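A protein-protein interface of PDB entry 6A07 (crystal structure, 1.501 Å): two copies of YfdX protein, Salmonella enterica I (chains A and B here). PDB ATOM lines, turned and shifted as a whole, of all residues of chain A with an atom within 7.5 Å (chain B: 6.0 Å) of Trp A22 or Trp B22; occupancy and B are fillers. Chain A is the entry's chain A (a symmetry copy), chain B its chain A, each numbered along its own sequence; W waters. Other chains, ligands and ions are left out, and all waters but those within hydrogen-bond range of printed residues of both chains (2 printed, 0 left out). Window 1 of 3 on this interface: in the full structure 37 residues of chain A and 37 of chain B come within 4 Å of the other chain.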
ATOM      1  N   ILE A  17     -12.738  14.387  -2.831  1.00  0.00           N
ATOM      2  CA  ILE A  17     -12.681  14.118  -1.394  1.00  0.00           C
ATOM      3  C   ILE A  17     -11.856  15.213  -0.736  1.00  0.00           C
ATOM      4  O   ILE A  17     -10.796  15.588  -1.255  1.00  0.00           O
ATOM      5  CB  ILE A  17     -12.052  12.736  -1.122  1.00  0.00           C
ATOM      6  CG1 ILE A  17     -12.842  11.618  -1.812  1.00  0.00           C
ATOM      7  CG2 ILE A  17     -11.961  12.484   0.377  1.00  0.00           C
ATOM      8  CD1 ILE A  17     -12.102  10.289  -1.838  1.00  0.00           C
ATOM      9  N   SER A  18     -12.323  15.732   0.403  1.00  0.00           N
ATOM     10  CA  SER A  18     -11.663  16.879   1.037  1.00  0.00           C
ATOM     11  C   SER A  18     -10.550  16.416   1.968  1.00  0.00           C
ATOM     12  O   SER A  18     -10.810  15.968   3.089  1.00  0.00           O
ATOM     13  CB  SER A  18     -12.651  17.748   1.806  1.00  0.00           C
ATOM     14  OG  SER A  18     -11.937  18.766   2.509  1.00  0.00           O
ATOM     15  N   GLY A  19      -9.303  16.577   1.530  1.00  0.00           N
ATOM     16  CA  GLY A  19      -8.194  16.296   2.423  1.00  0.00           C
ATOM     17  C   GLY A  19      -8.074  17.301   3.549  1.00  0.00           C
ATOM     18  O   GLY A  19      -7.589  16.962   4.636  1.00  0.00           O
ATOM     19  N   GLN A  20      -8.496  18.544   3.311  1.00  0.00           N
ATOM     20  CA  GLN A  20      -8.483  19.542   4.379  1.00  0.00           C
ATOM     21  C   GLN A  20      -9.431  19.147   5.500  1.00  0.00           C
ATOM     22  O   GLN A  20      -9.087  19.260   6.682  1.00  0.00           O
ATOM     23  CB  GLN A  20      -8.871  20.918   3.847  1.00  0.00           C
ATOM     24  CG  GLN A  20      -7.815  21.593   2.993  1.00  0.00           C
ATOM     25  CD  GLN A  20      -8.338  22.880   2.413  1.00  0.00           C
ATOM     26  OE1 GLN A  20      -9.375  22.890   1.746  1.00  0.00           O
ATOM     27  NE2 GLN A  20      -7.647  23.980   2.681  1.00  0.00           N
ATOM     28  N   ALA A  21     -10.636  18.692   5.147  1.00  0.00           N
ATOM     29  CA  ALA A  21     -11.596  18.321   6.183  1.00  0.00           C
ATOM     30  C   ALA A  21     -11.183  17.041   6.895  1.00  0.00           C
ATOM     31  O   ALA A  21     -11.473  16.875   8.088  1.00  0.00           O
ATOM     32  CB  ALA A  21     -12.998  18.174   5.589  1.00  0.00           C
ATOM     33  N   TRP A  22     -10.517  16.123   6.192  1.00  0.00           N
ATOM     34  CA  TRP A  22      -9.961  14.959   6.872  1.00  0.00           C
ATOM     35  C   TRP A  22      -8.945  15.394   7.922  1.00  0.00           C
ATOM     36  O   TRP A  22      -8.984  14.935   9.070  1.00  0.00           O
ATOM     37  CB  TRP A  22      -9.323  13.991   5.865  1.00  0.00           C
ATOM     38  CG  TRP A  22      -9.036  12.666   6.503  1.00  0.00           C
ATOM     39  CD1 TRP A  22      -9.897  11.611   6.634  1.00  0.00           C
ATOM     40  CD2 TRP A  22      -7.829  12.278   7.143  1.00  0.00           C
ATOM     41  NE1 TRP A  22      -9.289  10.578   7.303  1.00  0.00           N
ATOM     42  CE2 TRP A  22      -8.012  10.963   7.619  1.00  0.00           C
ATOM     43  CE3 TRP A  22      -6.596  12.907   7.340  1.00  0.00           C
ATOM     44  CZ2 TRP A  22      -7.019  10.274   8.291  1.00  0.00           C
ATOM     45  CZ3 TRP A  22      -5.611  12.221   8.008  1.00  0.00           C
ATOM     46  CH2 TRP A  22      -5.828  10.917   8.473  1.00  0.00           C
ATOM     47  N   GLN A  23      -8.027  16.289   7.548  1.00  0.00           N
ATOM     48  CA  GLN A  23      -7.032  16.743   8.510  1.00  0.00           C
ATOM     49  C   GLN A  23      -7.683  17.511   9.649  1.00  0.00           C
ATOM     50  O   GLN A  23      -7.220  17.430  10.794  1.00  0.00           O
ATOM     51  CB  GLN A  23      -5.984  17.608   7.811  1.00  0.00           C
ATOM     52  CG  GLN A  23      -4.822  18.039   8.710  1.00  0.00           C
ATOM     53  CD  GLN A  23      -4.040  16.854   9.219  1.00  0.00           C
ATOM     54  OE1 GLN A  23      -3.728  15.932   8.459  1.00  0.00           O
ATOM     55  NE2 GLN A  23      -3.747  16.846  10.511  1.00  0.00           N
ATOM     56  N   ALA A  24      -8.767  18.233   9.359  1.00  0.00           N
ATOM     57  CA  ALA A  24      -9.477  18.945  10.413  1.00  0.00           C
ATOM     58  C   ALA A  24     -10.034  17.971  11.437  1.00  0.00           C
ATOM     59  O   ALA A  24      -9.956  18.224  12.645  1.00  0.00           O
ATOM     60  CB  ALA A  24     -10.600  19.801   9.821  1.00  0.00           C
ATOM     61  N   MET A  25     -10.581  16.841  10.980  1.00  0.00           N
ATOM     62  CA  MET A  25     -11.115  15.873  11.937  1.00  0.00           C
ATOM     63  C   MET A  25      -9.995  15.257  12.763  1.00  0.00           C
ATOM     64  O   MET A  25     -10.170  14.996  13.959  1.00  0.00           O
ATOM     65  CB  MET A  25     -11.913  14.783  11.216  1.00  0.00           C
ATOM     66  CG  MET A  25     -13.141  15.278  10.479  1.00  0.00           C
ATOM     67  SD  MET A  25     -14.193  16.396  11.449  1.00  0.00           S
ATOM     68  CE  MET A  25     -14.712  15.308  12.774  1.00  0.00           C
ATOM     69  N   ARG A  26      -8.841  15.008  12.133  1.00  0.00           N
ATOM     70  CA  ARG A  26      -7.681  14.535  12.875  1.00  0.00           C
ATOM     71  C   ARG A  26      -7.284  15.558  13.938  1.00  0.00           C
ATOM     72  O   ARG A  26      -7.048  15.205  15.105  1.00  0.00           O
ATOM     73  CB  ARG A  26      -6.545  14.252  11.887  1.00  0.00           C
ATOM     74  CG  ARG A  26      -5.161  14.192  12.467  1.00  0.00           C
ATOM     75  CD  ARG A  26      -4.975  13.048  13.417  1.00  0.00           C
ATOM     76  NE  ARG A  26      -3.548  12.843  13.666  1.00  0.00           N
ATOM     77  CZ  ARG A  26      -3.060  12.084  14.640  1.00  0.00           C
ATOM     78  NH1 ARG A  26      -3.885  11.471  15.465  1.00  0.00           N
ATOM     79  NH2 ARG A  26      -1.747  11.948  14.790  1.00  0.00           N
ATOM     80  N   ASP A  27      -7.273  16.840  13.566  1.00  0.00           N
ATOM     81  CA  ASP A  27      -6.931  17.889  14.521  1.00  0.00           C
ATOM     82  C   ASP A  27      -7.940  17.970  15.668  1.00  0.00           C
ATOM     83  O   ASP A  27      -7.563  18.260  16.815  1.00  0.00           O
ATOM     84  CB  ASP A  27      -6.837  19.240  13.804  1.00  0.00           C
ATOM     85  CG  ASP A  27      -5.633  19.341  12.881  1.00  0.00           C
ATOM     86  OD1 ASP A  27      -4.739  18.469  12.933  1.00  0.00           O
ATOM     87  OD2 ASP A  27      -5.584  20.326  12.112  1.00  0.00           O
ATOM     88  N   ILE A  28      -9.227  17.773  15.365  1.00  0.00           N
ATOM     89  CA  ILE A  28     -10.276  17.803  16.388  1.00  0.00           C
ATOM     90  C   ILE A  28     -10.036  16.715  17.426  1.00  0.00           C
ATOM     91  O   ILE A  28     -10.155  16.951  18.637  1.00  0.00           O
ATOM     92  CB  ILE A  28     -11.658  17.680  15.714  1.00  0.00           C
ATOM     93  CG1 ILE A  28     -12.028  19.007  15.050  1.00  0.00           C
ATOM     94  CG2 ILE A  28     -12.750  17.241  16.690  1.00  0.00           C
ATOM     95  CD1 ILE A  28     -13.216  18.871  14.115  1.00  0.00           C
ATOM     96  N   MET A  30      -7.144  15.235  18.188  1.00  0.00           N
ATOM     97  CA  MET A  30      -5.932  15.531  18.943  1.00  0.00           C
ATOM     98  C   MET A  30      -6.194  16.666  19.924  1.00  0.00           C
ATOM     99  O   MET A  30      -5.715  16.633  21.061  1.00  0.00           O
ATOM    100  CB  MET A  30      -4.778  15.883  17.997  1.00  0.00           C
ATOM    101  CG  MET A  30      -4.345  14.748  17.059  1.00  0.00           C
ATOM    102  SD  MET A  30      -2.795  15.136  16.210  1.00  0.00           S
ATOM    103  CE  MET A  30      -1.982  15.902  17.623  1.00  0.00           C
ATOM    104  N   LEU A  53      -8.931  25.086   8.451  1.00  0.00           N
ATOM    105  CA  LEU A  53      -9.088  24.126   7.363  1.00  0.00           C
ATOM    106  C   LEU A  53     -10.536  24.037   6.899  1.00  0.00           C
ATOM    107  O   LEU A  53     -10.802  23.960   5.692  1.00  0.00           O
ATOM    108  CB  LEU A  53      -8.583  22.751   7.788  1.00  0.00           C
ATOM    109  CG  LEU A  53      -7.073  22.588   7.979  1.00  0.00           C
ATOM    110  CD1 LEU A  53      -6.748  21.370   8.815  1.00  0.00           C
ATOM    111  CD2 LEU A  53      -6.351  22.499   6.644  1.00  0.00           C
ATOM    112  N   LEU A  54     -11.488  24.013   7.838  1.00  0.00           N
ATOM    113  CA  LEU A  54     -12.886  23.849   7.465  1.00  0.00           C
ATOM    114  C   LEU A  54     -13.502  25.116   6.900  1.00  0.00           C
ATOM    115  O   LEU A  54     -14.573  25.049   6.286  1.00  0.00           O
ATOM    116  CB  LEU A  54     -13.705  23.397   8.679  1.00  0.00           C
ATOM    117  CG  LEU A  54     -13.416  21.982   9.172  1.00  0.00           C
ATOM    118  CD1 LEU A  54     -14.080  21.772  10.530  1.00  0.00           C
ATOM    119  CD2 LEU A  54     -13.893  20.934   8.164  1.00  0.00           C
ATOM    120  N   TRP A  61     -16.166  24.355  -1.465  1.00  0.00           N
ATOM    121  CA  TRP A  61     -16.717  23.247  -0.690  1.00  0.00           C
ATOM    122  C   TRP A  61     -17.800  22.486  -1.442  1.00  0.00           C
ATOM    123  O   TRP A  61     -18.056  21.318  -1.124  1.00  0.00           O
ATOM    124  CB  TRP A  61     -17.224  23.784   0.651  1.00  0.00           C
ATOM    125  CG  TRP A  61     -16.070  24.240   1.490  1.00  0.00           C
ATOM    126  CD1 TRP A  61     -15.657  25.531   1.708  1.00  0.00           C
ATOM    127  CD2 TRP A  61     -15.126  23.402   2.168  1.00  0.00           C
ATOM    128  NE1 TRP A  61     -14.527  25.540   2.489  1.00  0.00           N
ATOM    129  CE2 TRP A  61     -14.185  24.245   2.790  1.00  0.00           C
ATOM    130  CE3 TRP A  61     -14.988  22.014   2.313  1.00  0.00           C
ATOM    131  CZ2 TRP A  61     -13.121  23.748   3.549  1.00  0.00           C
ATOM    132  CZ3 TRP A  61     -13.935  21.524   3.071  1.00  0.00           C
ATOM    133  CH2 TRP A  61     -13.022  22.386   3.681  1.00  0.00           C
ATOM    134  N   ILE A  79     -20.153  16.274   3.453  1.00  0.00           N
ATOM    135  CA  ILE A  79     -19.033  16.269   2.517  1.00  0.00           C
ATOM    136  C   ILE A  79     -18.186  15.017   2.718  1.00  0.00           C
ATOM    137  O   ILE A  79     -18.076  14.476   3.825  1.00  0.00           O
ATOM    138  CB  ILE A  79     -18.153  17.533   2.629  1.00  0.00           C
ATOM    139  CG1 ILE A  79     -17.563  17.673   4.034  1.00  0.00           C
ATOM    140  CG2 ILE A  79     -18.947  18.785   2.201  1.00  0.00           C
ATOM    141  CD1 ILE A  79     -16.344  18.630   4.089  1.00  0.00           C
ATOM    142  N   ARG A  80     -17.547  14.588   1.629  1.00  0.00           N
ATOM    143  CA  ARG A  80     -16.675  13.415   1.637  1.00  0.00           C
ATOM    144  C   ARG A  80     -15.299  13.772   2.183  1.00  0.00           C
ATOM    145  O   ARG A  80     -14.672  14.745   1.729  1.00  0.00           O
ATOM    146  CB  ARG A  80     -16.507  12.858   0.221  1.00  0.00           C
ATOM    147  CG  ARG A  80     -17.775  12.318  -0.401  1.00  0.00           C
ATOM    148  CD  ARG A  80     -17.553  11.947  -1.866  1.00  0.00           C
ATOM    149  NE  ARG A  80     -17.350  13.145  -2.658  1.00  0.00           N
ATOM    150  CZ  ARG A  80     -18.329  13.817  -3.256  1.00  0.00           C
ATOM    151  NH1 ARG A  80     -19.595  13.385  -3.185  1.00  0.00           N
ATOM    152  NH2 ARG A  80     -18.032  14.926  -3.929  1.00  0.00           N
ATOM    153  N   ILE A  81     -14.803  12.977   3.131  1.00  0.00           N
ATOM    154  CA  ILE A  81     -13.471  13.204   3.688  1.00  0.00           C
ATOM    155  C   ILE A  81     -12.544  12.007   3.546  1.00  0.00           C
ATOM    156  O   ILE A  81     -11.335  12.164   3.756  1.00  0.00           O
ATOM    157  CB  ILE A  81     -13.529  13.658   5.169  1.00  0.00           C
ATOM    158  CG1 ILE A  81     -13.928  12.494   6.086  1.00  0.00           C
ATOM    159  CG2 ILE A  81     -14.465  14.861   5.328  1.00  0.00           C
ATOM    160  CD1 ILE A  81     -13.825  12.832   7.580  1.00  0.00           C
ATOM    161  N   ASN A  82     -13.050  10.828   3.181  1.00  0.00           N
ATOM    162  CA  ASN A  82     -12.181   9.681   2.951  1.00  0.00           C
ATOM    163  C   ASN A  82     -12.958   8.642   2.166  1.00  0.00           C
ATOM    164  O   ASN A  82     -14.185   8.604   2.226  1.00  0.00           O
ATOM    165  CB  ASN A  82     -11.667   9.083   4.265  1.00  0.00           C
ATOM    166  CG  ASN A  82     -10.560   8.076   4.040  1.00  0.00           C
ATOM    167  OD1 ASN A  82      -9.505   8.414   3.523  1.00  0.00           O
ATOM    168  ND2 ASN A  82     -10.815   6.818   4.399  1.00  0.00           N
ATOM    169  N   SER A  83     -12.232   7.811   1.416  1.00  0.00           N
ATOM    170  CA  SER A  83     -12.801   6.623   0.796  1.00  0.00           C
ATOM    171  C   SER A  83     -11.916   5.419   1.076  1.00  0.00           C
ATOM    172  O   SER A  83     -10.684   5.512   1.019  1.00  0.00           O
ATOM    173  CB  SER A  83     -12.946   6.797  -0.713  1.00  0.00           C
ATOM    174  OG  SER A  83     -14.173   6.268  -1.165  1.00  0.00           O
ATOM    175  N   GLU A 132     -16.408   8.090   3.969  1.00  0.00           N
ATOM    176  CA  GLU A 132     -16.499   8.752   5.260  1.00  0.00           C
ATOM    177  C   GLU A 132     -16.969  10.175   5.022  1.00  0.00           C
ATOM    178  O   GLU A 132     -16.383  10.886   4.199  1.00  0.00           O
ATOM    179  CB  GLU A 132     -15.136   8.740   5.949  1.00  0.00           C
ATOM    180  CG  GLU A 132     -15.177   9.145   7.391  1.00  0.00           C
ATOM    181  CD  GLU A 132     -13.805   9.279   8.041  1.00  0.00           C
ATOM    182  OE1 GLU A 132     -13.751   9.724   9.211  1.00  0.00           O
ATOM    183  OE2 GLU A 132     -12.793   8.965   7.392  1.00  0.00           O
ATOM    184  N   ILE A 134     -18.749  13.973   6.745  1.00  0.00           N
ATOM    185  CA  ILE A 134     -19.115  14.824   7.881  1.00  0.00           C
ATOM    186  C   ILE A 134     -20.111  15.886   7.440  1.00  0.00           C
ATOM    187  O   ILE A 134     -20.087  16.334   6.280  1.00  0.00           O
ATOM    188  CB  ILE A 134     -17.905  15.519   8.533  1.00  0.00           C
ATOM    189  CG1 ILE A 134     -17.159  16.384   7.517  1.00  0.00           C
ATOM    190  CG2 ILE A 134     -16.994  14.503   9.238  1.00  0.00           C
ATOM    191  CD1 ILE A 134     -16.155  17.324   8.175  1.00  0.00           C
ATOM    192  N   SER B  18       4.281   7.952  18.108  1.00  0.00           N
ATOM    193  CA  SER B  18       4.949   8.142  16.815  1.00  0.00           C
ATOM    194  C   SER B  18       4.001   8.770  15.802  1.00  0.00           C
ATOM    195  O   SER B  18       3.139   8.090  15.237  1.00  0.00           O
ATOM    196  CB  SER B  18       5.500   6.832  16.263  1.00  0.00           C
ATOM    197  OG  SER B  18       6.017   7.053  14.950  1.00  0.00           O
ATOM    198  N   GLY B  19       4.194  10.059  15.527  1.00  0.00           N
ATOM    199  CA  GLY B  19       3.425  10.682  14.466  1.00  0.00           C
ATOM    200  C   GLY B  19       3.813  10.188  13.088  1.00  0.00           C
ATOM    201  O   GLY B  19       2.978  10.175  12.175  1.00  0.00           O
ATOM    202  N   GLN B  20       5.074   9.789  12.911  1.00  0.00           N
ATOM    203  CA  GLN B  20       5.493   9.226  11.628  1.00  0.00           C
ATOM    204  C   GLN B  20       4.758   7.927  11.342  1.00  0.00           C
ATOM    205  O   GLN B  20       4.299   7.699  10.216  1.00  0.00           O
ATOM    206  CB  GLN B  20       6.997   8.974  11.607  1.00  0.00           C
ATOM    207  CG  GLN B  20       7.852  10.223  11.514  1.00  0.00           C
ATOM    208  CD  GLN B  20       9.314   9.880  11.629  1.00  0.00           C
ATOM    209  OE1 GLN B  20       9.734   9.250  12.601  1.00  0.00           O
ATOM    210  NE2 GLN B  20      10.097  10.265  10.630  1.00  0.00           N
ATOM    211  N   ALA B  21       4.645   7.056  12.347  1.00  0.00           N
ATOM    212  CA  ALA B  21       3.969   5.781  12.122  1.00  0.00           C
ATOM    213  C   ALA B  21       2.469   5.966  11.948  1.00  0.00           C
ATOM    214  O   ALA B  21       1.831   5.198  11.216  1.00  0.00           O
ATOM    215  CB  ALA B  21       4.260   4.809  13.266  1.00  0.00           C
ATOM    216  N   TRP B  22       1.883   6.965  12.612  1.00  0.00           N
ATOM    217  CA  TRP B  22       0.483   7.279  12.350  1.00  0.00           C
ATOM    218  C   TRP B  22       0.293   7.677  10.890  1.00  0.00           C
ATOM    219  O   TRP B  22      -0.615   7.182  10.212  1.00  0.00           O
ATOM    220  CB  TRP B  22      -0.011   8.392  13.286  1.00  0.00           C
ATOM    221  CG  TRP B  22      -1.505   8.503  13.246  1.00  0.00           C
ATOM    222  CD1 TRP B  22      -2.404   7.787  13.987  1.00  0.00           C
ATOM    223  CD2 TRP B  22      -2.269   9.336  12.387  1.00  0.00           C
ATOM    224  NE1 TRP B  22      -3.688   8.140  13.654  1.00  0.00           N
ATOM    225  CE2 TRP B  22      -3.630   9.098  12.675  1.00  0.00           C
ATOM    226  CE3 TRP B  22      -1.936  10.283  11.414  1.00  0.00           C
ATOM    227  CZ2 TRP B  22      -4.652   9.758  12.018  1.00  0.00           C
ATOM    228  CZ3 TRP B  22      -2.953  10.936  10.762  1.00  0.00           C
ATOM    229  CH2 TRP B  22      -4.295  10.672  11.069  1.00  0.00           C
ATOM    230  N   GLN B  23       1.151   8.568  10.385  1.00  0.00           N
ATOM    231  CA  GLN B  23       1.019   8.983   8.995  1.00  0.00           C
ATOM    232  C   GLN B  23       1.278   7.821   8.051  1.00  0.00           C
ATOM    233  O   GLN B  23       0.651   7.736   6.986  1.00  0.00           O
ATOM    234  CB  GLN B  23       1.977  10.137   8.700  1.00  0.00           C
ATOM    235  CG  GLN B  23       1.834  10.731   7.297  1.00  0.00           C
ATOM    236  CD  GLN B  23       0.464  11.325   7.079  1.00  0.00           C
ATOM    237  OE1 GLN B  23      -0.060  12.034   7.943  1.00  0.00           O
ATOM    238  NE2 GLN B  23      -0.143  11.017   5.942  1.00  0.00           N
ATOM    239  N   ALA B  24       2.174   6.908   8.434  1.00  0.00           N
ATOM    240  CA  ALA B  24       2.426   5.737   7.606  1.00  0.00           C
ATOM    241  C   ALA B  24       1.173   4.888   7.479  1.00  0.00           C
ATOM    242  O   ALA B  24       0.859   4.398   6.389  1.00  0.00           O
ATOM    243  CB  ALA B  24       3.578   4.909   8.184  1.00  0.00           C
ATOM    244  N   MET B  25       0.429   4.719   8.576  1.00  0.00           N
ATOM    245  CA  MET B  25      -0.793   3.921   8.489  1.00  0.00           C
ATOM    246  C   MET B  25      -1.832   4.618   7.623  1.00  0.00           C
ATOM    247  O   MET B  25      -2.570   3.959   6.879  1.00  0.00           O
ATOM    248  CB  MET B  25      -1.356   3.639   9.885  1.00  0.00           C
ATOM    249  CG  MET B  25      -0.451   2.819  10.782  1.00  0.00           C
ATOM    250  SD  MET B  25       0.241   1.339   9.990  1.00  0.00           S
ATOM    251  CE  MET B  25      -1.251   0.403   9.662  1.00  0.00           C
ATOM    252  N   ARG B  26      -1.910   5.950   7.721  1.00  0.00           N
ATOM    253  CA  ARG B  26      -2.789   6.704   6.839  1.00  0.00           C
ATOM    254  C   ARG B  26      -2.390   6.483   5.381  1.00  0.00           C
ATOM    255  O   ARG B  26      -3.244   6.214   4.520  1.00  0.00           O
ATOM    256  CB  ARG B  26      -2.738   8.182   7.239  1.00  0.00           C
ATOM    257  CG  ARG B  26      -3.205   9.165   6.204  1.00  0.00           C
ATOM    258  CD  ARG B  26      -4.663   9.030   5.884  1.00  0.00           C
ATOM    259  NE  ARG B  26      -5.118  10.213   5.154  1.00  0.00           N
ATOM    260  CZ  ARG B  26      -6.278  10.295   4.513  1.00  0.00           C
ATOM    261  NH1 ARG B  26      -7.091   9.259   4.500  1.00  0.00           N
ATOM    262  NH2 ARG B  26      -6.616  11.413   3.879  1.00  0.00           N
ATOM    263  N   ASP B  27      -1.086   6.525   5.101  1.00  0.00           N
ATOM    264  CA  ASP B  27      -0.608   6.301   3.740  1.00  0.00           C
ATOM    265  C   ASP B  27      -0.924   4.886   3.251  1.00  0.00           C
ATOM    266  O   ASP B  27      -1.212   4.686   2.059  1.00  0.00           O
ATOM    267  CB  ASP B  27       0.899   6.562   3.664  1.00  0.00           C
ATOM    268  CG  ASP B  27       1.256   8.032   3.813  1.00  0.00           C
ATOM    269  OD1 ASP B  27       0.354   8.896   3.766  1.00  0.00           O
ATOM    270  OD2 ASP B  27       2.466   8.314   3.959  1.00  0.00           O
ATOM    271  N   ILE B  81       0.913   4.820  18.278  1.00  0.00           N
ATOM    272  CA  ILE B  81       0.718   5.738  17.157  1.00  0.00           C
ATOM    273  C   ILE B  81      -0.392   6.751  17.390  1.00  0.00           C
ATOM    274  O   ILE B  81      -0.484   7.719  16.626  1.00  0.00           O
ATOM    275  CB  ILE B  81       0.480   4.985  15.823  1.00  0.00           C
ATOM    276  CG1 ILE B  81      -0.914   4.345  15.795  1.00  0.00           C
ATOM    277  CG2 ILE B  81       1.590   3.957  15.578  1.00  0.00           C
ATOM    278  CD1 ILE B  81      -1.280   3.742  14.431  1.00  0.00           C
ATOM    279  N   ASN B  82      -1.225   6.582  18.419  1.00  0.00           N
ATOM    280  CA  ASN B  82      -2.246   7.576  18.724  1.00  0.00           C
ATOM    281  C   ASN B  82      -2.739   7.337  20.138  1.00  0.00           C
ATOM    282  O   ASN B  82      -2.658   6.221  20.646  1.00  0.00           O
ATOM    283  CB  ASN B  82      -3.414   7.515  17.734  1.00  0.00           C
ATOM    284  CG  ASN B  82      -4.340   8.704  17.869  1.00  0.00           C
ATOM    285  OD1 ASN B  82      -3.933   9.839  17.662  1.00  0.00           O
ATOM    286  ND2 ASN B  82      -5.589   8.448  18.256  1.00  0.00           N
ATOM    287  N   GLU B 132      -3.627   3.523  20.484  1.00  0.00           N
ATOM    288  CA  GLU B 132      -3.593   2.803  19.222  1.00  0.00           C
ATOM    289  C   GLU B 132      -2.166   2.343  18.986  1.00  0.00           C
ATOM    290  O   GLU B 132      -1.239   3.155  19.059  1.00  0.00           O
ATOM    291  CB  GLU B 132      -4.062   3.715  18.090  1.00  0.00           C
ATOM    292  CG  GLU B 132      -4.329   3.000  16.801  1.00  0.00           C
ATOM    293  CD  GLU B 132      -4.651   3.922  15.630  1.00  0.00           C
ATOM    294  OE1 GLU B 132      -4.775   3.408  14.495  1.00  0.00           O
ATOM    295  OE2 GLU B 132      -4.763   5.143  15.833  1.00  0.00           O
HETATM  296  O   HOH W   1      -0.618  10.437  16.882  1.00  0.00           O
HETATM  297  O   HOH W   2      -9.009  11.652   2.415  1.00  0.00           O
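The guanidinium group (NH1) of Arg B26 is in hydrogen-bond range of the side-chain amide oxygen (OD1) of Asn A82 (2.7 Å).
OD1 of Asn B82 lies within hydrogen-bond range of NH1 of Arg A26 (2.7 Å).
SD of Met A30 lies close to NE of Arg A26 (3.5 Å).
N of Glu A132 is in hydrogen-bond range of O of Asn A82 (2.9 Å).
O of Asn B82 sits at hydrogen-bond distance from N of Glu B132 (2.9 Å).
Among the printed residues, pairs that only touch across the chains: Trp A22 with Trp B22 (3.0 Å), Trp A22 with Arg B26 (3.4 Å) and Arg A26 with Trp B22 (3.4 Å).
Trp A22 touches just these residues of chain B: Trp B22 and Arg B26.
Of the printed residues of chain B, Arg A26 touches Trp B22 and Asn B82.
Asp A27 touches none of the printed residues of chain B.
Printed residues of chain B within 4 Å of Asn A82: Arg B26.
Printed residues of chain A within 4 Å of Trp B22: Trp A22 and Arg A26.
Printed residues of chain A within 4 Å of Arg B26: Trp A22 and Asn A82.
Of the printed residues of chain A, Asn B82 touches Arg A26.
The nearest residue of chain B that does not touch Trp A22 is Gln B23 (5.6 Å).
The nearest residue of chain A that does not touch Trp B22 is Gln A23 (5.6 Å).
The nearest printed residue of chain A that does not touch Arg B26 is Ile A81 (4.8 Å).
Of the 23 printed residues of chain A, 3 touch a printed residue of chain B.
Hydrophobic or aromatic side chains of chain A that line the printed part of chain B: Trp A22.
Of the 13 printed residues of chain B, 3 touch a printed residue of chain A.
Printed residues of chain B that touch a printed residue of chain A: Trp B22, Arg B26 and Asn B82.
Trp B22 touches its own counterpart, Trp A22.
Trp A22 touches Arg B26, and with the chains exchanged Arg A26 touches Trp B22.
Arg A26 touches Asn B82, and with the chains exchanged Asn A82 touches Arg B26.
Positions printed for both chains: 18, 19, 20, 21, 22, 23, 24, 25, 26, 27, 81, 82 and 132.
Water W2 lies within hydrogen-bond range of the backbone carbonyl oxygen (O) of Ile A81, the guanidinium group (NH2) of Arg B26 and the side-chain amide oxygen (OD1) of Asn A82.
Water W1 lies within hydrogen-bond range of O of Ile B81 (2.7 Å), NH2 of Arg A26 (2.8 Å) and OD1 of Asn B82 (3.5 Å).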
